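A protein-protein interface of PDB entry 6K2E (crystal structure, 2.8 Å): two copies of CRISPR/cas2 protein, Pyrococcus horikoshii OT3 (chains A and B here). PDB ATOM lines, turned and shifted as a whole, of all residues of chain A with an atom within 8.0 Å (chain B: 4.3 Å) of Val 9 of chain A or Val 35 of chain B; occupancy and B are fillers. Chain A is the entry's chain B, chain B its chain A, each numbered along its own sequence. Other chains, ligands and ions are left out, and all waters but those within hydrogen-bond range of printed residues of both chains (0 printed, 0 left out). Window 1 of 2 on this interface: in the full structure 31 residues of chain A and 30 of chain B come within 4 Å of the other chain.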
ATOM      1  N   VAL A   6      34.976  -9.113 -18.104  1.00  0.00           N
ATOM      2  CA  VAL A   6      33.589  -9.470 -18.311  1.00  0.00           C
ATOM      3  C   VAL A   6      32.763  -9.015 -17.109  1.00  0.00           C
ATOM      4  O   VAL A   6      33.263  -8.933 -15.984  1.00  0.00           O
ATOM      5  CB  VAL A   6      33.505 -10.988 -18.594  1.00  0.00           C
ATOM      6  CG1 VAL A   6      33.456 -11.823 -17.344  1.00  0.00           C
ATOM      7  CG2 VAL A   6      32.383 -11.290 -19.487  1.00  0.00           C
ATOM      8  N   ILE A   7      31.504  -8.655 -17.364  1.00  0.00           N
ATOM      9  CA  ILE A   7      30.521  -8.406 -16.308  1.00  0.00           C
ATOM     10  C   ILE A   7      29.310  -9.271 -16.613  1.00  0.00           C
ATOM     11  O   ILE A   7      28.706  -9.140 -17.683  1.00  0.00           O
ATOM     12  CB  ILE A   7      30.086  -6.936 -16.220  1.00  0.00           C
ATOM     13  CG1 ILE A   7      31.249  -6.017 -15.889  1.00  0.00           C
ATOM     14  CG2 ILE A   7      28.988  -6.768 -15.176  1.00  0.00           C
ATOM     15  CD1 ILE A   7      30.856  -4.567 -16.009  1.00  0.00           C
ATOM     16  N   VAL A   8      28.957 -10.142 -15.675  1.00  0.00           N
ATOM     17  CA  VAL A   8      27.923 -11.154 -15.874  1.00  0.00           C
ATOM     18  C   VAL A   8      26.744 -10.879 -14.934  1.00  0.00           C
ATOM     19  O   VAL A   8      26.920 -10.816 -13.718  1.00  0.00           O
ATOM     20  CB  VAL A   8      28.505 -12.558 -15.661  1.00  0.00           C
ATOM     21  CG1 VAL A   8      27.439 -13.616 -15.752  1.00  0.00           C
ATOM     22  CG2 VAL A   8      29.595 -12.805 -16.674  1.00  0.00           C
ATOM     23  N   VAL A   9      25.542 -10.700 -15.477  1.00  0.00           N
ATOM     24  CA  VAL A   9      24.319 -10.582 -14.669  1.00  0.00           C
ATOM     25  C   VAL A   9      23.356 -11.727 -15.000  1.00  0.00           C
ATOM     26  O   VAL A   9      22.855 -11.808 -16.131  1.00  0.00           O
ATOM     27  CB  VAL A   9      23.612  -9.235 -14.899  1.00  0.00           C
ATOM     28  CG1 VAL A   9      22.553  -9.013 -13.839  1.00  0.00           C
ATOM     29  CG2 VAL A   9      24.631  -8.079 -14.959  1.00  0.00           C
ATOM     30  N   TYR A  10      23.017 -12.548 -14.001  1.00  0.00           N
ATOM     31  CA  TYR A  10      22.124 -13.678 -14.248  1.00  0.00           C
ATOM     32  C   TYR A  10      20.735 -13.462 -13.665  1.00  0.00           C
ATOM     33  O   TYR A  10      20.558 -12.822 -12.630  1.00  0.00           O
ATOM     34  CB  TYR A  10      22.678 -15.005 -13.705  1.00  0.00           C
ATOM     35  CG  TYR A  10      22.854 -15.128 -12.193  1.00  0.00           C
ATOM     36  CD1 TYR A  10      21.827 -15.603 -11.370  1.00  0.00           C
ATOM     37  CD2 TYR A  10      24.069 -14.851 -11.604  1.00  0.00           C
ATOM     38  CE1 TYR A  10      21.993 -15.730 -10.001  1.00  0.00           C
ATOM     39  CE2 TYR A  10      24.248 -14.992 -10.247  1.00  0.00           C
ATOM     40  CZ  TYR A  10      23.205 -15.434  -9.451  1.00  0.00           C
ATOM     41  OH  TYR A  10      23.399 -15.563  -8.101  1.00  0.00           O
ATOM     42  N   ASP A  11      19.756 -14.070 -14.311  1.00  0.00           N
ATOM     43  CA  ASP A  11      18.373 -14.060 -13.841  1.00  0.00           C
ATOM     44  C   ASP A  11      17.844 -15.482 -14.023  1.00  0.00           C
ATOM     45  O   ASP A  11      17.330 -15.837 -15.089  1.00  0.00           O
ATOM     46  CB  ASP A  11      17.545 -13.048 -14.600  1.00  0.00           C
ATOM     47  CG  ASP A  11      16.191 -12.888 -14.013  1.00  0.00           C
ATOM     48  OD1 ASP A  11      16.105 -12.202 -12.976  1.00  0.00           O
ATOM     49  OD2 ASP A  11      15.228 -13.459 -14.561  1.00  0.00           O
ATOM     50  N   VAL A  12      17.993 -16.294 -12.971  1.00  0.00           N
ATOM     51  CA  VAL A  12      17.729 -17.728 -12.995  1.00  0.00           C
ATOM     52  C   VAL A  12      16.718 -18.096 -11.907  1.00  0.00           C
ATOM     53  O   VAL A  12      16.751 -17.554 -10.799  1.00  0.00           O
ATOM     54  CB  VAL A  12      19.083 -18.466 -12.796  1.00  0.00           C
ATOM     55  CG1 VAL A  12      18.931 -19.949 -12.777  1.00  0.00           C
ATOM     56  CG2 VAL A  12      20.089 -18.080 -13.872  1.00  0.00           C
ATOM     57  N   VAL A  20      24.136 -22.129 -11.237  1.00  0.00           N
ATOM     58  CA  VAL A  20      24.666 -21.017 -12.019  1.00  0.00           C
ATOM     59  C   VAL A  20      25.657 -20.223 -11.172  1.00  0.00           C
ATOM     60  O   VAL A  20      26.736 -19.828 -11.641  1.00  0.00           O
ATOM     61  CB  VAL A  20      23.505 -20.146 -12.555  1.00  0.00           C
ATOM     62  CG1 VAL A  20      24.005 -18.908 -13.257  1.00  0.00           C
ATOM     63  CG2 VAL A  20      22.644 -20.955 -13.528  1.00  0.00           C
ATOM     64  N   LEU A  24      29.708 -19.821 -11.858  1.00  0.00           N
ATOM     65  CA  LEU A  24      30.274 -18.488 -12.023  1.00  0.00           C
ATOM     66  C   LEU A  24      31.302 -18.167 -10.955  1.00  0.00           C
ATOM     67  O   LEU A  24      32.163 -17.319 -11.191  1.00  0.00           O
ATOM     68  CB  LEU A  24      29.179 -17.425 -11.995  1.00  0.00           C
ATOM     69  CG  LEU A  24      28.353 -17.332 -13.265  1.00  0.00           C
ATOM     70  CD1 LEU A  24      27.045 -16.591 -12.993  1.00  0.00           C
ATOM     71  CD2 LEU A  24      29.158 -16.648 -14.350  1.00  0.00           C
ATOM     72  N   LEU A  28      34.952 -16.425 -11.872  1.00  0.00           N
ATOM     73  CA  LEU A  28      34.851 -14.982 -11.707  1.00  0.00           C
ATOM     74  C   LEU A  28      34.693 -14.614 -10.244  1.00  0.00           C
ATOM     75  O   LEU A  28      34.573 -15.475  -9.369  1.00  0.00           O
ATOM     76  CB  LEU A  28      33.692 -14.405 -12.524  1.00  0.00           C
ATOM     77  CG  LEU A  28      33.845 -14.474 -14.043  1.00  0.00           C
ATOM     78  CD1 LEU A  28      32.531 -14.220 -14.705  1.00  0.00           C
ATOM     79  CD2 LEU A  28      34.876 -13.497 -14.525  1.00  0.00           C
ATOM     80  N   GLN A  32      28.299  -8.668  -5.897  1.00  0.00           N
ATOM     81  CA  GLN A  32      27.149  -8.810  -5.032  1.00  0.00           C
ATOM     82  C   GLN A  32      26.026  -9.300  -5.935  1.00  0.00           C
ATOM     83  O   GLN A  32      26.269  -9.656  -7.100  1.00  0.00           O
ATOM     84  CB  GLN A  32      26.819  -7.550  -4.210  1.00  0.00           C
ATOM     85  CG  GLN A  32      26.471  -6.285  -4.918  1.00  0.00           C
ATOM     86  CD  GLN A  32      26.365  -5.197  -3.896  1.00  0.00           C
ATOM     87  OE1 GLN A  32      25.279  -4.801  -3.513  1.00  0.00           O
ATOM     88  NE2 GLN A  32      27.512  -4.752  -3.390  1.00  0.00           N
ATOM     89  N   ASN A  33      24.804  -9.092  -5.492  1.00  0.00           N
ATOM     90  CA  ASN A  33      23.671  -9.994  -5.540  1.00  0.00           C
ATOM     91  C   ASN A  33      23.648 -11.016  -6.670  1.00  0.00           C
ATOM     92  O   ASN A  33      23.812 -12.200  -6.395  1.00  0.00           O
ATOM     93  CB  ASN A  33      22.424  -9.082  -5.648  1.00  0.00           C
ATOM     94  CG  ASN A  33      22.565  -7.763  -4.809  1.00  0.00           C
ATOM     95  OD1 ASN A  33      22.429  -7.771  -3.578  1.00  0.00           O
ATOM     96  ND2 ASN A  33      22.846  -6.634  -5.495  1.00  0.00           N
ATOM     97  N   SER A  34      23.621 -10.609  -7.925  1.00  0.00           N
ATOM     98  CA  SER A  34      23.603 -11.599  -9.009  1.00  0.00           C
ATOM     99  C   SER A  34      24.578 -11.204 -10.096  1.00  0.00           C
ATOM    100  O   SER A  34      24.400 -11.561 -11.272  1.00  0.00           O
ATOM    101  CB  SER A  34      22.222 -11.789  -9.652  1.00  0.00           C
ATOM    102  OG  SER A  34      21.271 -12.256  -8.714  1.00  0.00           O
ATOM    103  N   VAL A  35      25.608 -10.458  -9.704  1.00  0.00           N
ATOM    104  CA  VAL A  35      26.580  -9.901 -10.622  1.00  0.00           C
ATOM    105  C   VAL A  35      27.946 -10.491 -10.323  1.00  0.00           C
ATOM    106  O   VAL A  35      28.420 -10.442  -9.182  1.00  0.00           O
ATOM    107  CB  VAL A  35      26.601  -8.369 -10.539  1.00  0.00           C
ATOM    108  CG1 VAL A  35      27.689  -7.818 -11.449  1.00  0.00           C
ATOM    109  CG2 VAL A  35      25.202  -7.810 -10.917  1.00  0.00           C
ATOM    110  N   PHE A  36      28.567 -11.062 -11.348  1.00  0.00           N
ATOM    111  CA  PHE A  36      29.935 -11.543 -11.289  1.00  0.00           C
ATOM    112  C   PHE A  36      30.767 -10.732 -12.272  1.00  0.00           C
ATOM    113  O   PHE A  36      30.240 -10.201 -13.255  1.00  0.00           O
ATOM    114  CB  PHE A  36      30.034 -13.021 -11.628  1.00  0.00           C
ATOM    115  CG  PHE A  36      29.651 -13.925 -10.509  1.00  0.00           C
ATOM    116  CD1 PHE A  36      28.317 -14.119 -10.180  1.00  0.00           C
ATOM    117  CD2 PHE A  36      30.615 -14.612  -9.800  1.00  0.00           C
ATOM    118  CE1 PHE A  36      27.962 -14.971  -9.147  1.00  0.00           C
ATOM    119  CE2 PHE A  36      30.253 -15.470  -8.767  1.00  0.00           C
ATOM    120  CZ  PHE A  36      28.930 -15.642  -8.439  1.00  0.00           C
ATOM    121  N   GLU A  37      32.056 -10.588 -11.976  1.00  0.00           N
ATOM    122  CA  GLU A  37      32.950  -9.879 -12.878  1.00  0.00           C
ATOM    123  C   GLU A  37      34.362 -10.404 -12.703  1.00  0.00           C
ATOM    124  O   GLU A  37      34.674 -11.113 -11.742  1.00  0.00           O
ATOM    125  CB  GLU A  37      32.899  -8.369 -12.660  1.00  0.00           C
ATOM    126  CG  GLU A  37      33.058  -7.951 -11.246  1.00  0.00           C
ATOM    127  CD  GLU A  37      33.071  -6.449 -11.103  1.00  0.00           C
ATOM    128  OE1 GLU A  37      34.017  -5.801 -11.593  1.00  0.00           O
ATOM    129  OE2 GLU A  37      32.126  -5.913 -10.495  1.00  0.00           O
ATOM    130  N   SER A  61      17.973 -16.271 -17.868  1.00  0.00           N
ATOM    131  CA  SER A  61      18.718 -15.343 -18.697  1.00  0.00           C
ATOM    132  C   SER A  61      20.051 -15.052 -18.020  1.00  0.00           C
ATOM    133  O   SER A  61      20.097 -14.831 -16.807  1.00  0.00           O
ATOM    134  CB  SER A  61      17.871 -14.082 -18.946  1.00  0.00           C
ATOM    135  OG  SER A  61      18.652 -12.917 -19.081  1.00  0.00           O
ATOM    136  N   VAL A  62      21.133 -15.093 -18.790  1.00  0.00           N
ATOM    137  CA  VAL A  62      22.438 -14.643 -18.324  1.00  0.00           C
ATOM    138  C   VAL A  62      22.957 -13.604 -19.301  1.00  0.00           C
ATOM    139  O   VAL A  62      23.142 -13.905 -20.485  1.00  0.00           O
ATOM    140  CB  VAL A  62      23.457 -15.793 -18.206  1.00  0.00           C
ATOM    141  CG1 VAL A  62      24.762 -15.260 -17.659  1.00  0.00           C
ATOM    142  CG2 VAL A  62      22.943 -16.913 -17.336  1.00  0.00           C
ATOM    143  N   LEU A  63      23.194 -12.391 -18.811  1.00  0.00           N
ATOM    144  CA  LEU A  63      23.806 -11.339 -19.599  1.00  0.00           C
ATOM    145  C   LEU A  63      25.310 -11.351 -19.397  1.00  0.00           C
ATOM    146  O   LEU A  63      25.790 -11.213 -18.271  1.00  0.00           O
ATOM    147  CB  LEU A  63      23.260  -9.978 -19.191  1.00  0.00           C
ATOM    148  CG  LEU A  63      21.774  -9.681 -19.332  1.00  0.00           C
ATOM    149  CD1 LEU A  63      21.554  -8.195 -19.164  1.00  0.00           C
ATOM    150  CD2 LEU A  63      21.245 -10.222 -20.662  1.00  0.00           C
ATOM    151  N   ILE A  64      26.054 -11.454 -20.490  1.00  0.00           N
ATOM    152  CA  ILE A  64      27.508 -11.476 -20.452  1.00  0.00           C
ATOM    153  C   ILE A  64      27.993 -10.273 -21.259  1.00  0.00           C
ATOM    154  O   ILE A  64      27.875 -10.253 -22.489  1.00  0.00           O
ATOM    155  CB  ILE A  64      28.063 -12.805 -20.993  1.00  0.00           C
ATOM    156  CG1 ILE A  64      27.554 -13.974 -20.137  1.00  0.00           C
ATOM    157  CG2 ILE A  64      29.571 -12.817 -21.007  1.00  0.00           C
ATOM    158  CD1 ILE A  64      28.140 -15.316 -20.487  1.00  0.00           C
ATOM    159  N   TYR A  65      28.498  -9.256 -20.559  1.00  0.00           N
ATOM    160  CA  TYR A  65      29.061  -8.052 -21.165  1.00  0.00           C
ATOM    161  C   TYR A  65      30.575  -8.220 -21.266  1.00  0.00           C
ATOM    162  O   TYR A  65      31.248  -8.368 -20.245  1.00  0.00           O
ATOM    163  CB  TYR A  65      28.742  -6.793 -20.347  1.00  0.00           C
ATOM    164  CG  TYR A  65      27.317  -6.313 -20.396  1.00  0.00           C
ATOM    165  CD1 TYR A  65      26.856  -5.524 -21.451  1.00  0.00           C
ATOM    166  CD2 TYR A  65      26.432  -6.640 -19.382  1.00  0.00           C
ATOM    167  CE1 TYR A  65      25.538  -5.088 -21.501  1.00  0.00           C
ATOM    168  CE2 TYR A  65      25.123  -6.209 -19.418  1.00  0.00           C
ATOM    169  CZ  TYR A  65      24.681  -5.433 -20.473  1.00  0.00           C
ATOM    170  OH  TYR A  65      23.376  -5.027 -20.484  1.00  0.00           O
ATOM    171  N   ILE B   7      26.062   1.088 -17.250  1.00  0.00           N
ATOM    172  CA  ILE B   7      25.267  -0.134 -17.119  1.00  0.00           C
ATOM    173  C   ILE B   7      24.816  -0.202 -15.671  1.00  0.00           C
ATOM    174  O   ILE B   7      25.648  -0.130 -14.761  1.00  0.00           O
ATOM    175  CB  ILE B   7      26.045  -1.414 -17.478  1.00  0.00           C
ATOM    176  CG1 ILE B   7      26.535  -1.410 -18.909  1.00  0.00           C
ATOM    177  CG2 ILE B   7      25.169  -2.651 -17.301  1.00  0.00           C
ATOM    178  CD1 ILE B   7      27.451  -2.598 -19.185  1.00  0.00           C
ATOM    179  N   VAL B   8      23.508  -0.272 -15.457  1.00  0.00           N
ATOM    180  CA  VAL B   8      22.897  -0.202 -14.130  1.00  0.00           C
ATOM    181  C   VAL B   8      22.199  -1.520 -13.831  1.00  0.00           C
ATOM    182  O   VAL B   8      21.334  -1.957 -14.598  1.00  0.00           O
ATOM    183  CB  VAL B   8      21.916   0.974 -14.004  1.00  0.00           C
ATOM    184  CG1 VAL B   8      21.073   0.834 -12.766  1.00  0.00           C
ATOM    185  CG2 VAL B   8      22.682   2.284 -13.974  1.00  0.00           C
ATOM    186  N   VAL B   9      22.596  -2.169 -12.738  1.00  0.00           N
ATOM    187  CA  VAL B   9      21.916  -3.354 -12.228  1.00  0.00           C
ATOM    188  C   VAL B   9      21.393  -3.020 -10.842  1.00  0.00           C
ATOM    189  O   VAL B   9      22.180  -2.645  -9.963  1.00  0.00           O
ATOM    190  CB  VAL B   9      22.848  -4.576 -12.171  1.00  0.00           C
ATOM    191  CG1 VAL B   9      22.044  -5.816 -12.048  1.00  0.00           C
ATOM    192  CG2 VAL B   9      23.758  -4.646 -13.399  1.00  0.00           C
ATOM    193  N   TRP B  30      16.019   0.303 -21.273  1.00  0.00           N
ATOM    194  CA  TRP B  30      15.757  -0.956 -20.589  1.00  0.00           C
ATOM    195  C   TRP B  30      16.260  -2.121 -21.427  1.00  0.00           C
ATOM    196  O   TRP B  30      15.732  -2.386 -22.514  1.00  0.00           O
ATOM    197  CB  TRP B  30      14.268  -1.080 -20.319  1.00  0.00           C
ATOM    198  CG  TRP B  30      13.932  -2.217 -19.499  1.00  0.00           C
ATOM    199  CD1 TRP B  30      14.735  -2.843 -18.601  1.00  0.00           C
ATOM    200  CD2 TRP B  30      12.696  -2.892 -19.479  1.00  0.00           C
ATOM    201  NE1 TRP B  30      14.079  -3.873 -18.014  1.00  0.00           N
ATOM    202  CE2 TRP B  30      12.813  -3.927 -18.534  1.00  0.00           C
ATOM    203  CE3 TRP B  30      11.484  -2.723 -20.161  1.00  0.00           C
ATOM    204  CZ2 TRP B  30      11.765  -4.788 -18.254  1.00  0.00           C
ATOM    205  CZ3 TRP B  30      10.434  -3.595 -19.876  1.00  0.00           C
ATOM    206  CH2 TRP B  30      10.586  -4.607 -18.936  1.00  0.00           C
ATOM    207  N   ARG B  31      17.302  -2.796 -20.939  1.00  0.00           N
ATOM    208  CA  ARG B  31      17.834  -3.967 -21.628  1.00  0.00           C
ATOM    209  C   ARG B  31      16.989  -5.198 -21.342  1.00  0.00           C
ATOM    210  O   ARG B  31      16.320  -5.736 -22.231  1.00  0.00           O
ATOM    211  CB  ARG B  31      19.293  -4.201 -21.196  1.00  0.00           C
ATOM    212  CG  ARG B  31      19.928  -5.536 -21.584  1.00  0.00           C
ATOM    213  CD  ARG B  31      19.969  -5.703 -23.079  1.00  0.00           C
ATOM    214  NE  ARG B  31      20.981  -4.860 -23.691  1.00  0.00           N
ATOM    215  CZ  ARG B  31      21.145  -4.737 -24.998  1.00  0.00           C
ATOM    216  NH1 ARG B  31      20.351  -5.401 -25.830  1.00  0.00           N
ATOM    217  NH2 ARG B  31      22.107  -3.957 -25.468  1.00  0.00           N
ATOM    218  N   GLN B  32      16.991  -5.630 -20.088  1.00  0.00           N
ATOM    219  CA  GLN B  32      16.242  -6.770 -19.622  1.00  0.00           C
ATOM    220  C   GLN B  32      16.120  -6.584 -18.113  1.00  0.00           C
ATOM    221  O   GLN B  32      16.671  -5.645 -17.575  1.00  0.00           O
ATOM    222  CB  GLN B  32      16.984  -8.055 -20.005  1.00  0.00           C
ATOM    223  CG  GLN B  32      16.129  -9.188 -20.342  1.00  0.00           C
ATOM    224  CD  GLN B  32      16.875 -10.274 -21.042  1.00  0.00           C
ATOM    225  OE1 GLN B  32      16.981 -11.383 -20.528  1.00  0.00           O
ATOM    226  NE2 GLN B  32      17.416  -9.965 -22.229  1.00  0.00           N
ATOM    227  N   ASN B  33      15.678  -7.656 -17.455  1.00  0.00           N
ATOM    228  CA  ASN B  33      14.910  -7.683 -16.215  1.00  0.00           C
ATOM    229  C   ASN B  33      15.161  -6.535 -15.240  1.00  0.00           C
ATOM    230  O   ASN B  33      14.264  -5.745 -14.913  1.00  0.00           O
ATOM    231  CB  ASN B  33      15.226  -9.011 -15.506  1.00  0.00           C
ATOM    232  CG  ASN B  33      15.272 -10.199 -16.470  1.00  0.00           C
ATOM    233  OD1 ASN B  33      16.327 -10.516 -17.022  1.00  0.00           O
ATOM    234  ND2 ASN B  33      14.132 -10.854 -16.679  1.00  0.00           N
ATOM    235  N   SER B  34      16.404  -6.369 -14.848  1.00  0.00           N
ATOM    236  CA  SER B  34      16.731  -5.308 -13.913  1.00  0.00           C
ATOM    237  C   SER B  34      18.017  -4.599 -14.341  1.00  0.00           C
ATOM    238  O   SER B  34      18.703  -3.980 -13.516  1.00  0.00           O
ATOM    239  CB  SER B  34      16.793  -5.890 -12.501  1.00  0.00           C
ATOM    240  OG  SER B  34      17.735  -5.222 -11.699  1.00  0.00           O
ATOM    241  N   VAL B  35      18.316  -4.651 -15.641  1.00  0.00           N
ATOM    242  CA  VAL B  35      19.515  -4.081 -16.239  1.00  0.00           C
ATOM    243  C   VAL B  35      19.092  -2.949 -17.172  1.00  0.00           C
ATOM    244  O   VAL B  35      18.218  -3.134 -18.030  1.00  0.00           O
ATOM    245  CB  VAL B  35      20.331  -5.138 -16.994  1.00  0.00           C
ATOM    246  CG1 VAL B  35      21.521  -4.473 -17.697  1.00  0.00           C
ATOM    247  CG2 VAL B  35      20.802  -6.229 -16.021  1.00  0.00           C
ATOM    248  N   PHE B  36      19.651  -1.764 -16.945  1.00  0.00           N
ATOM    249  CA  PHE B  36      19.467  -0.606 -17.806  1.00  0.00           C
ATOM    250  C   PHE B  36      20.816  -0.135 -18.337  1.00  0.00           C
ATOM    251  O   PHE B  36      21.840  -0.232 -17.650  1.00  0.00           O
ATOM    252  CB  PHE B  36      18.810   0.539 -17.050  1.00  0.00           C
ATOM    253  CG  PHE B  36      17.337   0.370 -16.835  1.00  0.00           C
ATOM    254  CD1 PHE B  36      16.855  -0.430 -15.807  1.00  0.00           C
ATOM    255  CD2 PHE B  36      16.431   1.036 -17.648  1.00  0.00           C
ATOM    256  CE1 PHE B  36      15.482  -0.573 -15.613  1.00  0.00           C
ATOM    257  CE2 PHE B  36      15.072   0.894 -17.461  1.00  0.00           C
ATOM    258  CZ  PHE B  36      14.596   0.094 -16.455  1.00  0.00           C
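Of the 21 printed residues of chain A, 6 touch a printed residue of chain B. Printed residues of chain A that touch a printed residue of chain B: Val 9, Asp 11, Val 35, Ser 61, Leu 63 and Tyr 65. Hydrophobic or aromatic side chains of chain A that line the printed part of chain B: Val 9, Val 35, Leu 63 and Tyr 65. Hydrophobic or aromatic side chains of chain B within 4 Å of the printed part of chain A: Ile 7, Val 9 and Val 35. Among the printed residues, 11 pairs touch across the chains. Among the printed residues, no Asp or Glu carboxylate lies within 4 Å of a Lys or Arg side-chain nitrogen of the other chain.
Val 9 of chain B touches Val 9 of chain A. Val 9 of chain A touches Val 35 of chain B. Asn 33 of chain B touches Asp 11 of chain A. Val 9 of chain B touches Val 35 of chain A (CG1 to CG2, 3.9 Å). Ser 61 of chain A touches Asn 33 of chain B (OG to OD1, 3.9 Å). Leu 63 of chain A touches Arg 31 of chain B (CD1 to CG, 3.9 Å). Leu 63 of chain A touches Val 35 of chain B. Tyr 65 of chain A touches Ile 7 of chain B (CD1 to CD1, 3.7 Å). Tyr 65 of chain A touches Arg 31 of chain B. Val 35 of chain B touches Tyr 65 of chain A.
The side-chain amide oxygen (OE1) of Gln 32 of chain B lies within hydrogen-bond range of the side-chain hydroxyl (OG) of Ser 61 of chain A, at 2.7 Å.
Val 9 of chain B touches its own counterpart, Val 9 of chain A. Val 9 of chain A touches Val 35 of chain B, and with the chains exchanged Val 35 of chain A touches Val 9 of chain B. Positions printed for both chains: 7, 8, 9, 32, 33, 34, 35 and 36. Of the 11 pairs that touch across the chains among the printed residues, 3 have their exchanged pair printed and touching as well.
Val 9 of chain A touches just these residues of chain B: Val 9 (3.7 Å) and Val 35 (3.9 Å). Of chain A, only Val 9 (3.9 Å), Leu 63 (3.8 Å) and Tyr 65 (3.4 Å) come within 4 Å of Val 35 of chain B. Of the printed residues of chain A, Arg 31 of chain B touches Leu 63 and Tyr 65. Of the printed residues of chain A, Asn 33 of chain B touches Asp 11 (3.5 Å) and Ser 61 (3.9 Å). Val 12 of chain A touches none of the printed residues of chain B. The nearest residue of chain A that does not touch Val 35 of chain B is Val 35 of chain A (6.9 Å). The nearest printed residue of chain A that does not touch Gln 32 of chain B is Leu 63 of chain A (4.1 Å).
O of Gln 32 of chain B is in hydrogen-bond range of NE1 of Trp 30 of chain B (3.2 Å). The backbone carbonyl oxygen of Ile 7 of chain A sits at hydrogen-bond distance from the backbone NH of Tyr 65 of chain A, 2.9 Å away. O of Val 9 of chain A sits at hydrogen-bond distance from N of Leu 63 of chain A, 2.8 Å away. The backbone NH (N) of Asp 11 of chain A lies within hydrogen-bond range of the backbone carbonyl oxygen (O) of Ser 61 of chain A, 2.6 Å away.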
